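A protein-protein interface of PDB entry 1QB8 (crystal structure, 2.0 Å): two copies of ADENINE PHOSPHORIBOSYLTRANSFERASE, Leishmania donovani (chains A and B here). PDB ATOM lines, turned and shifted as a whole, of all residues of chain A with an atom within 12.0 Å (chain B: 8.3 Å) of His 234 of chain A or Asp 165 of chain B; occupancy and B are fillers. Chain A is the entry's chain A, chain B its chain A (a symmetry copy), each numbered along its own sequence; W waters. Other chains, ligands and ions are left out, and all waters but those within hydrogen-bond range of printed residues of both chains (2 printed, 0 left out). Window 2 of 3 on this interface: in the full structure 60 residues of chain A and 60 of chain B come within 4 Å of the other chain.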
ATOM      1  N   LEU A 225      32.128  31.470   1.410  1.00  0.00           N
ATOM      2  CA  LEU A 225      32.668  30.133   1.676  1.00  0.00           C
ATOM      3  C   LEU A 225      32.969  29.417   0.360  1.00  0.00           C
ATOM      4  O   LEU A 225      32.214  29.544  -0.600  1.00  0.00           O
ATOM      5  CB  LEU A 225      31.642  29.307   2.460  1.00  0.00           C
ATOM      6  CG  LEU A 225      31.189  29.872   3.805  1.00  0.00           C
ATOM      7  CD1 LEU A 225      29.957  29.135   4.302  1.00  0.00           C
ATOM      8  CD2 LEU A 225      32.333  29.783   4.808  1.00  0.00           C
ATOM      9  N   SER A 226      34.059  28.658   0.315  1.00  0.00           N
ATOM     10  CA  SER A 226      34.417  27.928  -0.898  1.00  0.00           C
ATOM     11  C   SER A 226      33.549  26.685  -1.013  1.00  0.00           C
ATOM     12  O   SER A 226      32.937  26.262  -0.033  1.00  0.00           O
ATOM     13  CB  SER A 226      35.885  27.518  -0.860  1.00  0.00           C
ATOM     14  OG  SER A 226      36.118  26.627   0.216  1.00  0.00           O
ATOM     15  N   CYS A 227      33.488  26.106  -2.207  1.00  0.00           N
ATOM     16  CA  CYS A 227      32.707  24.893  -2.423  1.00  0.00           C
ATOM     17  C   CYS A 227      33.203  23.777  -1.520  1.00  0.00           C
ATOM     18  O   CYS A 227      32.407  23.070  -0.910  1.00  0.00           O
ATOM     19  CB  CYS A 227      32.831  24.432  -3.864  1.00  0.00           C
ATOM     20  SG  CYS A 227      31.925  25.425  -4.993  1.00  0.00           S
ATOM     21  N   GLY A 228      34.525  23.631  -1.447  1.00  0.00           N
ATOM     22  CA  GLY A 228      35.131  22.603  -0.619  1.00  0.00           C
ATOM     23  C   GLY A 228      34.739  22.674   0.844  1.00  0.00           C
ATOM     24  O   GLY A 228      34.503  21.647   1.478  1.00  0.00           O
ATOM     25  N   ASP A 229      34.672  23.880   1.396  1.00  0.00           N
ATOM     26  CA  ASP A 229      34.293  24.042   2.795  1.00  0.00           C
ATOM     27  C   ASP A 229      32.832  23.677   3.043  1.00  0.00           C
ATOM     28  O   ASP A 229      32.502  23.086   4.074  1.00  0.00           O
ATOM     29  CB  ASP A 229      34.586  25.465   3.274  1.00  0.00           C
ATOM     30  CG  ASP A 229      36.076  25.732   3.427  1.00  0.00           C
ATOM     31  OD1 ASP A 229      36.443  26.694   4.131  1.00  0.00           O
ATOM     32  OD2 ASP A 229      36.886  24.972   2.850  1.00  0.00           O
ATOM     33  N   VAL A 230      31.966  24.010   2.090  1.00  0.00           N
ATOM     34  CA  VAL A 230      30.549  23.697   2.215  1.00  0.00           C
ATOM     35  C   VAL A 230      30.345  22.189   2.052  1.00  0.00           C
ATOM     36  O   VAL A 230      29.521  21.593   2.749  1.00  0.00           O
ATOM     37  CB  VAL A 230      29.699  24.476   1.186  1.00  0.00           C
ATOM     38  CG1 VAL A 230      28.234  24.105   1.322  1.00  0.00           C
ATOM     39  CG2 VAL A 230      29.871  25.971   1.397  1.00  0.00           C
ATOM     40  N   LEU A 231      31.114  21.571   1.153  1.00  0.00           N
ATOM     41  CA  LEU A 231      31.023  20.129   0.920  1.00  0.00           C
ATOM     42  C   LEU A 231      31.356  19.352   2.193  1.00  0.00           C
ATOM     43  O   LEU A 231      30.789  18.292   2.450  1.00  0.00           O
ATOM     44  CB  LEU A 231      31.969  19.695  -0.202  1.00  0.00           C
ATOM     45  CG  LEU A 231      31.471  19.752  -1.646  1.00  0.00           C
ATOM     46  CD1 LEU A 231      32.604  19.383  -2.587  1.00  0.00           C
ATOM     47  CD2 LEU A 231      30.305  18.797  -1.832  1.00  0.00           C
ATOM     48  N   ALA A 232      32.252  19.909   3.002  1.00  0.00           N
ATOM     49  CA  ALA A 232      32.672  19.287   4.251  1.00  0.00           C
ATOM     50  C   ALA A 232      31.619  19.345   5.365  1.00  0.00           C
ATOM     51  O   ALA A 232      31.773  18.695   6.403  1.00  0.00           O
ATOM     52  CB  ALA A 232      33.975  19.925   4.721  1.00  0.00           C
ATOM     53  N   GLU A 233      30.557  20.122   5.152  1.00  0.00           N
ATOM     54  CA  GLU A 233      29.487  20.270   6.143  1.00  0.00           C
ATOM     55  C   GLU A 233      28.428  19.180   6.038  1.00  0.00           C
ATOM     56  O   GLU A 233      27.491  19.140   6.841  1.00  0.00           O
ATOM     57  CB  GLU A 233      28.791  21.624   5.992  1.00  0.00           C
ATOM     58  CG  GLU A 233      29.706  22.832   6.006  1.00  0.00           C
ATOM     59  CD  GLU A 233      28.942  24.148   6.014  1.00  0.00           C
ATOM     60  OE1 GLU A 233      29.560  25.185   6.333  1.00  0.00           O
ATOM     61  OE2 GLU A 233      27.726  24.150   5.710  1.00  0.00           O
ATOM     62  N   HIS A 234      28.554  18.320   5.033  1.00  0.00           N
ATOM     63  CA  HIS A 234      27.591  17.245   4.834  1.00  0.00           C
ATOM     64  C   HIS A 234      28.231  15.997   4.211  1.00  0.00           C
ATOM     65  O   HIS A 234      29.254  16.086   3.533  1.00  0.00           O
ATOM     66  CB  HIS A 234      26.401  17.740   3.986  1.00  0.00           C
ATOM     67  CG  HIS A 234      26.776  18.202   2.608  1.00  0.00           C
ATOM     68  ND1 HIS A 234      26.877  19.537   2.272  1.00  0.00           N
ATOM     69  CD2 HIS A 234      27.047  17.508   1.477  1.00  0.00           C
ATOM     70  CE1 HIS A 234      27.193  19.643   0.993  1.00  0.00           C
ATOM     71  NE2 HIS A 234      27.302  18.427   0.488  1.00  0.00           N
ATOM     72  N   PRO A 235      27.658  14.809   4.488  1.00  0.00           N
ATOM     73  CA  PRO A 235      28.149  13.528   3.968  1.00  0.00           C
ATOM     74  C   PRO A 235      28.090  13.425   2.440  1.00  0.00           C
ATOM     75  O   PRO A 235      27.044  13.651   1.828  1.00  0.00           O
ATOM     76  CB  PRO A 235      27.217  12.509   4.630  1.00  0.00           C
ATOM     77  CG  PRO A 235      26.855  13.167   5.920  1.00  0.00           C
ATOM     78  CD  PRO A 235      26.588  14.583   5.479  1.00  0.00           C
ATOM     79  N   HIS A 236      29.226  13.096   1.835  1.00  0.00           N
ATOM     80  CA  HIS A 236      29.327  12.949   0.385  1.00  0.00           C
ATOM     81  C   HIS A 236      30.531  12.079  -0.001  1.00  0.00           C
ATOM     82  O   HIS A 236      30.658  11.741  -1.200  1.00  0.00           O
ATOM     83  CB  HIS A 236      29.424  14.328  -0.295  1.00  0.00           C
ATOM     84  CG  HIS A 236      30.735  15.027  -0.087  1.00  0.00           C
ATOM     85  ND1 HIS A 236      31.119  15.553   1.129  1.00  0.00           N
ATOM     86  CD2 HIS A 236      31.747  15.293  -0.947  1.00  0.00           C
ATOM     87  CE1 HIS A 236      32.310  16.114   1.009  1.00  0.00           C
ATOM     88  NE2 HIS A 236      32.712  15.970  -0.241  1.00  0.00           N
ATOM     89  OXT HIS A 236      31.341  11.746   0.897  1.00  0.00           O
ATOM     90  N   ILE B 111      28.553  31.052  -1.580  1.00  0.00           N
ATOM     91  CA  ILE B 111      29.375  29.864  -1.816  1.00  0.00           C
ATOM     92  C   ILE B 111      30.126  30.207  -3.103  1.00  0.00           C
ATOM     93  O   ILE B 111      29.499  30.595  -4.084  1.00  0.00           O
ATOM     94  CB  ILE B 111      28.516  28.602  -2.111  1.00  0.00           C
ATOM     95  CG1 ILE B 111      27.507  28.358  -0.989  1.00  0.00           C
ATOM     96  CG2 ILE B 111      29.415  27.371  -2.277  1.00  0.00           C
ATOM     97  CD1 ILE B 111      26.580  27.195  -1.254  1.00  0.00           C
ATOM     98  N   TYR B 132      24.202  30.978  -0.289  1.00  0.00           N
ATOM     99  CA  TYR B 132      24.161  29.750   0.486  1.00  0.00           C
ATOM    100  C   TYR B 132      22.701  29.469   0.824  1.00  0.00           C
ATOM    101  O   TYR B 132      22.013  30.334   1.353  1.00  0.00           O
ATOM    102  CB  TYR B 132      24.975  29.940   1.770  1.00  0.00           C
ATOM    103  CG  TYR B 132      25.012  28.734   2.677  1.00  0.00           C
ATOM    104  CD1 TYR B 132      23.997  28.501   3.610  1.00  0.00           C
ATOM    105  CD2 TYR B 132      26.077  27.835   2.624  1.00  0.00           C
ATOM    106  CE1 TYR B 132      24.044  27.402   4.472  1.00  0.00           C
ATOM    107  CE2 TYR B 132      26.137  26.732   3.482  1.00  0.00           C
ATOM    108  CZ  TYR B 132      25.118  26.522   4.402  1.00  0.00           C
ATOM    109  OH  TYR B 132      25.185  25.440   5.254  1.00  0.00           O
ATOM    110  N   ILE B 135      19.778  26.988  -3.127  1.00  0.00           N
ATOM    111  CA  ILE B 135      19.480  25.686  -3.710  1.00  0.00           C
ATOM    112  C   ILE B 135      19.705  24.678  -2.600  1.00  0.00           C
ATOM    113  O   ILE B 135      20.790  24.606  -2.035  1.00  0.00           O
ATOM    114  CB  ILE B 135      20.416  25.363  -4.888  1.00  0.00           C
ATOM    115  CG1 ILE B 135      20.196  26.368  -6.021  1.00  0.00           C
ATOM    116  CG2 ILE B 135      20.147  23.964  -5.402  1.00  0.00           C
ATOM    117  CD1 ILE B 135      21.255  26.312  -7.108  1.00  0.00           C
ATOM    118  N   GLY B 136      18.670  23.914  -2.274  1.00  0.00           N
ATOM    119  CA  GLY B 136      18.792  22.944  -1.203  1.00  0.00           C
ATOM    120  C   GLY B 136      19.057  21.498  -1.584  1.00  0.00           C
ATOM    121  O   GLY B 136      19.113  21.130  -2.761  1.00  0.00           O
ATOM    122  N   LYS B 137      19.253  20.684  -0.552  1.00  0.00           N
ATOM    123  CA  LYS B 137      19.487  19.256  -0.709  1.00  0.00           C
ATOM    124  C   LYS B 137      18.306  18.655  -1.481  1.00  0.00           C
ATOM    125  O   LYS B 137      17.149  18.992  -1.228  1.00  0.00           O
ATOM    126  CB  LYS B 137      19.601  18.616   0.679  1.00  0.00           C
ATOM    127  CG  LYS B 137      19.799  17.113   0.688  1.00  0.00           C
ATOM    128  CD  LYS B 137      19.963  16.618   2.113  1.00  0.00           C
ATOM    129  CE  LYS B 137      20.158  15.113   2.154  1.00  0.00           C
ATOM    130  NZ  LYS B 137      20.245  14.602   3.557  1.00  0.00           N
ATOM    131  N   GLY B 138      18.608  17.830  -2.475  1.00  0.00           N
ATOM    132  CA  GLY B 138      17.554  17.210  -3.254  1.00  0.00           C
ATOM    133  C   GLY B 138      17.042  18.014  -4.435  1.00  0.00           C
ATOM    134  O   GLY B 138      16.219  17.514  -5.206  1.00  0.00           O
ATOM    135  N   SER B 139      17.508  19.253  -4.584  1.00  0.00           N
ATOM    136  CA  SER B 139      17.083  20.095  -5.703  1.00  0.00           C
ATOM    137  C   SER B 139      17.592  19.526  -7.024  1.00  0.00           C
ATOM    138  O   SER B 139      18.610  18.833  -7.068  1.00  0.00           O
ATOM    139  CB  SER B 139      17.601  21.530  -5.545  1.00  0.00           C
ATOM    140  OG  SER B 139      17.170  22.116  -4.326  1.00  0.00           O
ATOM    141  N   ARG B 140      16.841  19.791  -8.085  1.00  0.00           N
ATOM    142  CA  ARG B 140      17.184  19.347  -9.431  1.00  0.00           C
ATOM    143  C   ARG B 140      17.247  20.653 -10.221  1.00  0.00           C
ATOM    144  O   ARG B 140      16.227  21.278 -10.520  1.00  0.00           O
ATOM    145  CB  ARG B 140      16.119  18.375  -9.955  1.00  0.00           C
ATOM    146  CG  ARG B 140      15.972  17.129  -9.055  1.00  0.00           C
ATOM    147  CD  ARG B 140      14.935  16.129  -9.556  1.00  0.00           C
ATOM    148  NE  ARG B 140      13.559  16.629  -9.495  1.00  0.00           N
ATOM    149  CZ  ARG B 140      12.806  16.666  -8.397  1.00  0.00           C
ATOM    150  NH1 ARG B 140      13.294  16.245  -7.239  1.00  0.00           N
ATOM    151  NH2 ARG B 140      11.537  17.057  -8.474  1.00  0.00           N
ATOM    152  N   VAL B 141      18.475  21.068 -10.507  1.00  0.00           N
ATOM    153  CA  VAL B 141      18.758  22.333 -11.162  1.00  0.00           C
ATOM    154  C   VAL B 141      19.127  22.305 -12.631  1.00  0.00           C
ATOM    155  O   VAL B 141      20.004  21.545 -13.057  1.00  0.00           O
ATOM    156  CB  VAL B 141      19.922  23.044 -10.428  1.00  0.00           C
ATOM    157  CG1 VAL B 141      20.051  24.492 -10.885  1.00  0.00           C
ATOM    158  CG2 VAL B 141      19.730  22.962  -8.921  1.00  0.00           C
ATOM    159  N   LEU B 158      28.328  23.662 -12.113  1.00  0.00           N
ATOM    160  CA  LEU B 158      28.356  22.283 -11.622  1.00  0.00           C
ATOM    161  C   LEU B 158      28.888  22.212 -10.189  1.00  0.00           C
ATOM    162  O   LEU B 158      28.271  21.604  -9.317  1.00  0.00           O
ATOM    163  CB  LEU B 158      29.222  21.402 -12.532  1.00  0.00           C
ATOM    164  CG  LEU B 158      28.880  21.357 -14.027  1.00  0.00           C
ATOM    165  CD1 LEU B 158      29.891  20.484 -14.771  1.00  0.00           C
ATOM    166  CD2 LEU B 158      27.469  20.835 -14.226  1.00  0.00           C
ATOM    167  N   GLN B 159      30.022  22.859  -9.943  1.00  0.00           N
ATOM    168  CA  GLN B 159      30.617  22.856  -8.610  1.00  0.00           C
ATOM    169  C   GLN B 159      29.666  23.395  -7.552  1.00  0.00           C
ATOM    170  O   GLN B 159      29.541  22.818  -6.474  1.00  0.00           O
ATOM    171  CB  GLN B 159      31.901  23.682  -8.592  1.00  0.00           C
ATOM    172  CG  GLN B 159      33.032  23.108  -9.420  1.00  0.00           C
ATOM    173  CD  GLN B 159      34.239  24.018  -9.453  1.00  0.00           C
ATOM    174  OE1 GLN B 159      34.131  25.223  -9.224  1.00  0.00           O
ATOM    175  NE2 GLN B 159      35.397  23.452  -9.773  1.00  0.00           N
ATOM    176  N   LEU B 160      28.992  24.499  -7.863  1.00  0.00           N
ATOM    177  CA  LEU B 160      28.064  25.123  -6.921  1.00  0.00           C
ATOM    178  C   LEU B 160      26.827  24.272  -6.616  1.00  0.00           C
ATOM    179  O   LEU B 160      26.378  24.220  -5.474  1.00  0.00           O
ATOM    180  CB  LEU B 160      27.669  26.524  -7.405  1.00  0.00           C
ATOM    181  CG  LEU B 160      28.846  27.498  -7.437  1.00  0.00           C
ATOM    182  CD1 LEU B 160      28.487  28.759  -8.188  1.00  0.00           C
ATOM    183  CD2 LEU B 160      29.287  27.817  -6.020  1.00  0.00           C
ATOM    184  N   VAL B 161      26.283  23.607  -7.631  1.00  0.00           N
ATOM    185  CA  VAL B 161      25.114  22.748  -7.438  1.00  0.00           C
ATOM    186  C   VAL B 161      25.547  21.513  -6.635  1.00  0.00           C
ATOM    187  O   VAL B 161      24.854  21.069  -5.714  1.00  0.00           O
ATOM    188  CB  VAL B 161      24.492  22.331  -8.799  1.00  0.00           C
ATOM    189  CG1 VAL B 161      23.405  21.292  -8.593  1.00  0.00           C
ATOM    190  CG2 VAL B 161      23.917  23.544  -9.498  1.00  0.00           C
ATOM    191  N   GLU B 162      26.730  21.005  -6.963  1.00  0.00           N
ATOM    192  CA  GLU B 162      27.305  19.855  -6.279  1.00  0.00           C
ATOM    193  C   GLU B 162      27.536  20.185  -4.807  1.00  0.00           C
ATOM    194  O   GLU B 162      27.090  19.456  -3.925  1.00  0.00           O
ATOM    195  CB  GLU B 162      28.625  19.478  -6.944  1.00  0.00           C
ATOM    196  CG  GLU B 162      29.428  18.428  -6.211  1.00  0.00           C
ATOM    197  CD  GLU B 162      30.684  18.049  -6.967  1.00  0.00           C
ATOM    198  OE1 GLU B 162      31.510  18.950  -7.255  1.00  0.00           O
ATOM    199  OE2 GLU B 162      30.833  16.849  -7.288  1.00  0.00           O
ATOM    200  N   ALA B 163      28.198  21.311  -4.552  1.00  0.00           N
ATOM    201  CA  ALA B 163      28.488  21.767  -3.193  1.00  0.00           C
ATOM    202  C   ALA B 163      27.219  21.979  -2.358  1.00  0.00           C
ATOM    203  O   ALA B 163      27.259  21.913  -1.132  1.00  0.00           O
ATOM    204  CB  ALA B 163      29.298  23.055  -3.243  1.00  0.00           C
ATOM    205  N   SER B 164      26.103  22.242  -3.031  1.00  0.00           N
ATOM    206  CA  SER B 164      24.822  22.473  -2.370  1.00  0.00           C
ATOM    207  C   SER B 164      24.068  21.186  -2.081  1.00  0.00           C
ATOM    208  O   SER B 164      22.948  21.222  -1.576  1.00  0.00           O
ATOM    209  CB  SER B 164      23.945  23.382  -3.232  1.00  0.00           C
ATOM    210  OG  SER B 164      24.541  24.655  -3.382  1.00  0.00           O
ATOM    211  N   ASP B 165      24.673  20.056  -2.429  1.00  0.00           N
ATOM    212  CA  ASP B 165      24.069  18.747  -2.212  1.00  0.00           C
ATOM    213  C   ASP B 165      22.833  18.575  -3.104  1.00  0.00           C
ATOM    214  O   ASP B 165      21.837  17.966  -2.710  1.00  0.00           O
ATOM    215  CB  ASP B 165      23.716  18.575  -0.725  1.00  0.00           C
ATOM    216  CG  ASP B 165      23.796  17.124  -0.257  1.00  0.00           C
ATOM    217  OD1 ASP B 165      24.250  16.245  -1.032  1.00  0.00           O
ATOM    218  OD2 ASP B 165      23.408  16.868   0.908  1.00  0.00           O
ATOM    219  N   ALA B 166      22.918  19.113  -4.316  1.00  0.00           N
ATOM    220  CA  ALA B 166      21.831  19.037  -5.291  1.00  0.00           C
ATOM    221  C   ALA B 166      22.363  18.405  -6.573  1.00  0.00           C
ATOM    222  O   ALA B 166      23.562  18.196  -6.703  1.00  0.00           O
ATOM    223  CB  ALA B 166      21.290  20.438  -5.579  1.00  0.00           C
ATOM    224  N   VAL B 167      21.479  18.090  -7.514  1.00  0.00           N
ATOM    225  CA  VAL B 167      21.924  17.496  -8.778  1.00  0.00           C
ATOM    226  C   VAL B 167      21.617  18.379  -9.991  1.00  0.00           C
ATOM    227  O   VAL B 167      20.648  19.144  -9.992  1.00  0.00           O
ATOM    228  CB  VAL B 167      21.337  16.057  -9.017  1.00  0.00           C
ATOM    229  CG1 VAL B 167      21.798  15.105  -7.921  1.00  0.00           C
ATOM    230  CG2 VAL B 167      19.819  16.088  -9.095  1.00  0.00           C
ATOM    231  N   VAL B 168      22.484  18.294 -10.997  1.00  0.00           N
ATOM    232  CA  VAL B 168      22.317  19.050 -12.229  1.00  0.00           C
ATOM    233  C   VAL B 168      21.463  18.236 -13.188  1.00  0.00           C
ATOM    234  O   VAL B 168      21.733  17.056 -13.423  1.00  0.00           O
ATOM    235  CB  VAL B 168      23.679  19.360 -12.906  1.00  0.00           C
ATOM    236  CG1 VAL B 168      23.469  19.993 -14.274  1.00  0.00           C
ATOM    237  CG2 VAL B 168      24.488  20.305 -12.044  1.00  0.00           C
HETATM  238  O   HOH W   1      24.432  14.262   1.549  1.00  0.00           O
HETATM  239  O   HOH W   2      27.421  16.949  -2.358  1.00  0.00           O
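Water W1 bridges the backbone carbonyl oxygen of Pro 235 of chain A (2.7 Å) and the side-chain carboxylate of Asp 165 of chain B (2.9 Å).
Water W2 lies within hydrogen-bond range of the backbone carbonyl oxygen of Glu 162 of chain B and a ring nitrogen (NE2) of His 234 of chain A.
Of the 12 printed residues of chain A, 6 touch a printed residue of chain B.
Printed residues of chain A that touch a printed residue of chain B: Leu 225, Cys 227, Val 230, Leu 231, Glu 233 and His 234.
Hydrophobic or aromatic side chains of chain A within 4 Å of the printed part of chain B: Val 230, Leu 231 and His 234.
Along chain A the printed residues that touch a printed residue of chain B span positions 225 to 234.
Asp 165 of chain B touches just one residue of chain A: His 234.
No residue of chain B comes within 4 Å of Pro 235 of chain A.
No residue of chain A comes within 4 Å of Lys 137 of chain B.
No residue of chain A comes within 4 Å of Gly 138 of chain B.
No residue of chain A comes within 4 Å of Ser 139 of chain B.
No residue of chain A comes within 4 Å of Val 161 of chain B.
Ala 163 of chain B touches just these residues of chain A: Cys 227 (3.8 Å), Val 230 (3.4 Å), Leu 231 (3.7 Å) and His 234 (3.1 Å).
No residue of chain A comes within 4 Å of Ser 164 of chain B.
No residue of chain A comes within 4 Å of Val 167 of chain B.
Printed residues of chain A within 4 Å of Leu 160 of chain B: Cys 227 (3.7 Å).
Printed residues of chain B within 4 Å of Leu 231 of chain A: Glu 162 (3.9 Å) and Ala 163 (3.7 Å).
Ile 135 of chain B touches none of the printed residues of chain A.
His 236 of chain A touches none of the printed residues of chain B.
The nearest residue of chain B that does not touch His 234 of chain A is Glu 162 of chain B (4.5 Å).
The nearest residue of chain A that does not touch Asp 165 of chain B is Pro 235 of chain A (4.8 Å).
Among the printed residues, pairs that only touch across the chains: Leu 225 of chain A with Ile 111 of chain B, His 234 of chain A with Ala 163 of chain B, Val 230 of chain A with Ala 163 of chain B, His 234 of chain A with Asp 165 of chain B, Cys 227 of chain A with Leu 160 of chain B, Leu 231 of chain A with Ala 163 of chain B, Cys 227 of chain A with Gln 159 of chain B, Cys 227 of chain A with Ala 163 of chain B, Leu 231 of chain A with Glu 162 of chain B, Val 230 of chain A with Ile 111 of chain B and Val 230 of chain A with Tyr 132 of chain B.
The side-chain hydroxyl (OH) of Tyr 132 of chain B sits at hydrogen-bond distance from the side-chain carboxylate (OE2) of Glu 233 of chain A (2.9 Å).
No position is printed for both chains.
Of the 12 pairs that touch across the chains among the printed residues, none has its exchanged pair printed and touching as well.
ND1 of His 234 of chain A sits at hydrogen-bond distance from O of Val 230 of chain A (3.4 Å).
O of Leu 231 of chain A lies close to ND1 of His 236 of chain A, at 3.1 Å.
The backbone carbonyl oxygen of His 234 of chain A sits at hydrogen-bond distance from a ring nitrogen (ND1) of His 236 of chain A.
The backbone NH (N) of Gly 138 of chain B is in hydrogen-bond range of the backbone carbonyl oxygen (O) of Asp 165 of chain B (3.2 Å).
The side-chain hydroxyl (OG) of Ser 164 of chain B sits at hydrogen-bond distance from the backbone carbonyl oxygen (O) of Leu 160 of chain B (2.8 Å).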
